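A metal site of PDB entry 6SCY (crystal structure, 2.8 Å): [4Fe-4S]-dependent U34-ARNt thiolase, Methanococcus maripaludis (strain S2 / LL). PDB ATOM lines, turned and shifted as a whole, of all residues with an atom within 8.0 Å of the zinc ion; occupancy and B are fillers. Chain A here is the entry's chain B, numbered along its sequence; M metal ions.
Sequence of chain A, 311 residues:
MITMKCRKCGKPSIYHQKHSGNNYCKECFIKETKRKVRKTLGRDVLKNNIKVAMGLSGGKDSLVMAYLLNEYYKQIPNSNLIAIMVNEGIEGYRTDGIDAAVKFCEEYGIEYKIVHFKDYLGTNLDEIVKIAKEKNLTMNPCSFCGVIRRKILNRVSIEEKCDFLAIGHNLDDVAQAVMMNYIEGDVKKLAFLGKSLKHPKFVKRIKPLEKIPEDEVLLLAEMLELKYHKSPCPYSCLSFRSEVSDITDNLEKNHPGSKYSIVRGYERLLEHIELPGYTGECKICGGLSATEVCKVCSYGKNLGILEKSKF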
ATOM      1  N   LYS A 151      17.851 -11.108  -3.362  1.00  0.00           N
ATOM      2  CA  LYS A 151      16.736 -10.416  -3.998  1.00  0.00           C
ATOM      3  C   LYS A 151      17.157  -9.769  -5.325  1.00  0.00           C
ATOM      4  O   LYS A 151      16.353  -9.752  -6.257  1.00  0.00           O
ATOM      5  CB  LYS A 151      16.105  -9.396  -3.030  1.00  0.00           C
ATOM      6  CG  LYS A 151      14.690  -9.004  -3.412  1.00  0.00           C
ATOM      7  CD  LYS A 151      13.915  -8.413  -2.246  1.00  0.00           C
ATOM      8  CE  LYS A 151      12.773  -7.536  -2.676  1.00  0.00           C
ATOM      9  NZ  LYS A 151      11.756  -8.267  -3.482  1.00  0.00           N
ATOM     10  N   GLU A 281       3.182 -11.777  -2.079  1.00  0.00           N
ATOM     11  CA  GLU A 281       2.760 -10.915  -0.973  1.00  0.00           C
ATOM     12  C   GLU A 281       3.880 -10.012  -0.437  1.00  0.00           C
ATOM     13  O   GLU A 281       4.803 -10.500   0.218  1.00  0.00           O
ATOM     14  CB  GLU A 281       2.102 -11.740   0.159  1.00  0.00           C
ATOM     15  CG  GLU A 281       0.949 -12.642  -0.271  1.00  0.00           C
ATOM     16  CD  GLU A 281      -0.321 -11.991  -0.808  1.00  0.00           C
ATOM     17  OE1 GLU A 281      -1.062 -12.675  -1.556  1.00  0.00           O
ATOM     18  OE2 GLU A 281      -0.588 -10.809  -0.480  1.00  0.00           O
ATOM     19  N   CYS A 282       3.781  -8.695  -0.742  1.00  0.00           N
ATOM     20  CA  CYS A 282       4.713  -7.614  -0.348  1.00  0.00           C
ATOM     21  C   CYS A 282       4.168  -6.229  -0.748  1.00  0.00           C
ATOM     22  O   CYS A 282       3.224  -6.130  -1.543  1.00  0.00           O
ATOM     23  CB  CYS A 282       6.106  -7.849  -0.936  1.00  0.00           C
ATOM     24  SG  CYS A 282       7.399  -6.833  -0.189  1.00  0.00           S
ATOM     25  N   LYS A 283       4.774  -5.152  -0.194  1.00  0.00           N
ATOM     26  CA  LYS A 283       4.423  -3.766  -0.483  1.00  0.00           C
ATOM     27  C   LYS A 283       5.499  -3.095  -1.349  1.00  0.00           C
ATOM     28  O   LYS A 283       6.694  -3.311  -1.111  1.00  0.00           O
ATOM     29  CB  LYS A 283       4.212  -2.969   0.816  1.00  0.00           C
ATOM     30  CG  LYS A 283       2.898  -3.275   1.532  1.00  0.00           C
ATOM     31  CD  LYS A 283       2.766  -2.501   2.831  1.00  0.00           C
ATOM     32  CE  LYS A 283       1.484  -2.804   3.549  1.00  0.00           C
ATOM     33  NZ  LYS A 283       1.409  -2.114   4.860  1.00  0.00           N
ATOM     34  N   ILE A 284       5.063  -2.293  -2.344  1.00  0.00           N
ATOM     35  CA  ILE A 284       5.859  -1.500  -3.302  1.00  0.00           C
ATOM     36  C   ILE A 284       6.734  -2.396  -4.234  1.00  0.00           C
ATOM     37  O   ILE A 284       6.458  -2.420  -5.437  1.00  0.00           O
ATOM     38  CB  ILE A 284       6.691  -0.338  -2.656  1.00  0.00           C
ATOM     39  CG1 ILE A 284       5.758   0.647  -1.898  1.00  0.00           C
ATOM     40  CG2 ILE A 284       7.539   0.407  -3.700  1.00  0.00           C
ATOM     41  CD1 ILE A 284       6.351   1.275  -0.639  1.00  0.00           C
ATOM     42  N   CYS A 285       7.762  -3.109  -3.698  1.00  0.00           N
ATOM     43  CA  CYS A 285       8.684  -3.945  -4.470  1.00  0.00           C
ATOM     44  C   CYS A 285       8.061  -5.246  -5.032  1.00  0.00           C
ATOM     45  O   CYS A 285       7.378  -5.200  -6.055  1.00  0.00           O
ATOM     46  CB  CYS A 285       9.975  -4.226  -3.707  1.00  0.00           C
ATOM     47  SG  CYS A 285       9.724  -4.825  -2.008  1.00  0.00           S
ATOM     48  N   GLY A 286       8.380  -6.382  -4.409  1.00  0.00           N
ATOM     49  CA  GLY A 286       7.903  -7.695  -4.846  1.00  0.00           C
ATOM     50  C   GLY A 286       7.900  -8.755  -3.772  1.00  0.00           C
ATOM     51  O   GLY A 286       8.706  -8.702  -2.838  1.00  0.00           O
ATOM     52  N   GLY A 287       6.985  -9.706  -3.921  1.00  0.00           N
ATOM     53  CA  GLY A 287       6.739 -10.814  -3.011  1.00  0.00           C
ATOM     54  C   GLY A 287       7.929 -11.679  -2.648  1.00  0.00           C
ATOM     55  O   GLY A 287       8.821 -11.907  -3.473  1.00  0.00           O
ATOM     56  N   LEU A 288       7.924 -12.160  -1.399  1.00  0.00           N
ATOM     57  CA  LEU A 288       8.931 -13.055  -0.819  1.00  0.00           C
ATOM     58  C   LEU A 288       8.235 -14.020   0.146  1.00  0.00           C
ATOM     59  O   LEU A 288       8.528 -15.220   0.132  1.00  0.00           O
ATOM     60  CB  LEU A 288      10.042 -12.248  -0.104  1.00  0.00           C
ATOM     61  CG  LEU A 288      11.251 -13.036   0.430  1.00  0.00           C
ATOM     62  CD1 LEU A 288      12.338 -13.173  -0.629  1.00  0.00           C
ATOM     63  CD2 LEU A 288      11.829 -12.370   1.662  1.00  0.00           C
ATOM     64  N   ALA A 290       5.183 -12.531   3.098  1.00  0.00           N
ATOM     65  CA  ALA A 290       3.973 -11.793   3.482  1.00  0.00           C
ATOM     66  C   ALA A 290       4.189 -10.291   3.370  1.00  0.00           C
ATOM     67  O   ALA A 290       5.322  -9.815   3.424  1.00  0.00           O
ATOM     68  CB  ALA A 290       3.576 -12.164   4.895  1.00  0.00           C
ATOM     69  N   THR A 291       3.078  -9.543   3.190  1.00  0.00           N
ATOM     70  CA  THR A 291       3.058  -8.082   3.080  1.00  0.00           C
ATOM     71  C   THR A 291       3.641  -7.464   4.367  1.00  0.00           C
ATOM     72  O   THR A 291       4.804  -7.049   4.336  1.00  0.00           O
ATOM     73  CB  THR A 291       1.659  -7.549   2.651  1.00  0.00           C
ATOM     74  OG1 THR A 291       1.595  -6.132   2.847  1.00  0.00           O
ATOM     75  CG2 THR A 291       0.491  -8.224   3.371  1.00  0.00           C
ATOM     76  N   VAL A 293       5.442  -5.843   6.879  1.00  0.00           N
ATOM     77  CA  VAL A 293       6.516  -4.846   6.759  1.00  0.00           C
ATOM     78  C   VAL A 293       7.637  -5.699   6.144  1.00  0.00           C
ATOM     79  O   VAL A 293       8.033  -6.698   6.755  1.00  0.00           O
ATOM     80  CB  VAL A 293       6.944  -4.199   8.124  1.00  0.00           C
ATOM     81  CG1 VAL A 293       8.172  -3.311   7.948  1.00  0.00           C
ATOM     82  CG2 VAL A 293       5.802  -3.398   8.752  1.00  0.00           C
ATOM     83  N   CYS A 294       8.073  -5.359   4.909  1.00  0.00           N
ATOM     84  CA  CYS A 294       9.082  -6.145   4.205  1.00  0.00           C
ATOM     85  C   CYS A 294      10.398  -6.252   4.968  1.00  0.00           C
ATOM     86  O   CYS A 294      10.948  -5.243   5.412  1.00  0.00           O
ATOM     87  CB  CYS A 294       9.296  -5.640   2.782  1.00  0.00           C
ATOM     88  SG  CYS A 294      10.526  -6.585   1.843  1.00  0.00           S
ATOM     89  N   LYS A 295      10.893  -7.499   5.111  1.00  0.00           N
ATOM     90  CA  LYS A 295      12.122  -7.897   5.816  1.00  0.00           C
ATOM     91  C   LYS A 295      13.359  -7.232   5.221  1.00  0.00           C
ATOM     92  O   LYS A 295      14.295  -6.922   5.960  1.00  0.00           O
ATOM     93  CB  LYS A 295      12.283  -9.438   5.865  1.00  0.00           C
ATOM     94  CG  LYS A 295      11.105 -10.274   5.349  1.00  0.00           C
ATOM     95  CD  LYS A 295       9.977 -10.463   6.378  1.00  0.00           C
ATOM     96  CE  LYS A 295       8.723 -11.028   5.767  1.00  0.00           C
ATOM     97  NZ  LYS A 295       7.550 -10.913   6.672  1.00  0.00           N
ATOM     98  N   VAL A 296      13.357  -7.005   3.893  1.00  0.00           N
ATOM     99  CA  VAL A 296      14.439  -6.349   3.149  1.00  0.00           C
ATOM    100  C   VAL A 296      14.260  -4.833   3.308  1.00  0.00           C
ATOM    101  O   VAL A 296      15.239  -4.124   3.548  1.00  0.00           O
ATOM    102  CB  VAL A 296      14.465  -6.758   1.646  1.00  0.00           C
ATOM    103  CG1 VAL A 296      15.688  -6.189   0.926  1.00  0.00           C
ATOM    104  CG2 VAL A 296      14.400  -8.267   1.473  1.00  0.00           C
ATOM    105  N   CYS A 297      12.994  -4.358   3.204  1.00  0.00           N
ATOM    106  CA  CYS A 297      12.623  -2.941   3.328  1.00  0.00           C
ATOM    107  C   CYS A 297      12.555  -2.457   4.782  1.00  0.00           C
ATOM    108  O   CYS A 297      12.176  -1.318   5.021  1.00  0.00           O
ATOM    109  CB  CYS A 297      11.337  -2.650   2.578  1.00  0.00           C
ATOM    110  SG  CYS A 297      11.372  -3.166   0.841  1.00  0.00           S
ATOM    111  N   SER A 298      12.933  -3.335   5.753  1.00  0.00           N
ATOM    112  CA  SER A 298      12.983  -3.043   7.179  1.00  0.00           C
ATOM    113  C   SER A 298      14.107  -2.028   7.436  1.00  0.00           C
ATOM    114  O   SER A 298      13.920  -1.076   8.184  1.00  0.00           O
ATOM    115  CB  SER A 298      13.243  -4.339   7.960  1.00  0.00           C
ATOM    116  OG  SER A 298      13.480  -4.112   9.343  1.00  0.00           O
ATOM    117  N   ILE A 305      13.006   4.471   0.986  1.00  0.00           N
ATOM    118  CA  ILE A 305      12.750   3.537  -0.116  1.00  0.00           C
ATOM    119  C   ILE A 305      13.239   4.100  -1.459  1.00  0.00           C
ATOM    120  O   ILE A 305      12.945   5.247  -1.801  1.00  0.00           O
ATOM    121  CB  ILE A 305      11.250   3.089  -0.157  1.00  0.00           C
ATOM    122  CG1 ILE A 305      10.693   2.694   1.256  1.00  0.00           C
ATOM    123  CG2 ILE A 305      10.976   1.995  -1.202  1.00  0.00           C
ATOM    124  CD1 ILE A 305      11.399   1.476   2.014  1.00  0.00           C
ATOM    125  N   SER A 309      10.851  -1.678  -8.654  1.00  0.00           N
ATOM    126  CA  SER A 309       9.675  -2.317  -8.056  1.00  0.00           C
ATOM    127  C   SER A 309       8.695  -2.832  -9.138  1.00  0.00           C
ATOM    128  O   SER A 309       8.862  -2.515 -10.321  1.00  0.00           O
ATOM    129  CB  SER A 309       8.961  -1.316  -7.144  1.00  0.00           C
ATOM    130  OG  SER A 309       9.728  -1.028  -5.988  1.00  0.00           O
HETATM  131 ZN    ZN M   1       9.874  -5.803  -0.082  1.00  0.00          ZN
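SG of Cys 297 sits close to SG of Cys 285 (3.7 Å).
The side-chain sulfur (SG) of Cys 285 sits close to the backbone carbonyl oxygen (O) of Lys 283, 3.5 Å away.
The side-chain sulfur of Cys 294 sits close to the backbone NH of Cys 297.
N of Val 296 sits close to SG of Cys 294.
The side-chain sulfur (SG) of Cys 282 sits close to the backbone carbonyl oxygen (O) of Gly 286 (3.5 Å).
SG of Cys 297 touches the zinc ion, 3.2 Å away.
Four residues have an atom within 4 Å of the zinc ion: Cys 282, Cys 285, Cys 294 and Cys 297.
The side-chain sulfur (SG) of Cys 285 is bound to the zinc ion (2.2 Å).
The zinc ion is bound by SG of Cys 294 (2.2 Å).
The zinc ion is bound by SG of Cys 282 (2.7 Å).
The zinc ion has three donor atoms within binding distance.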
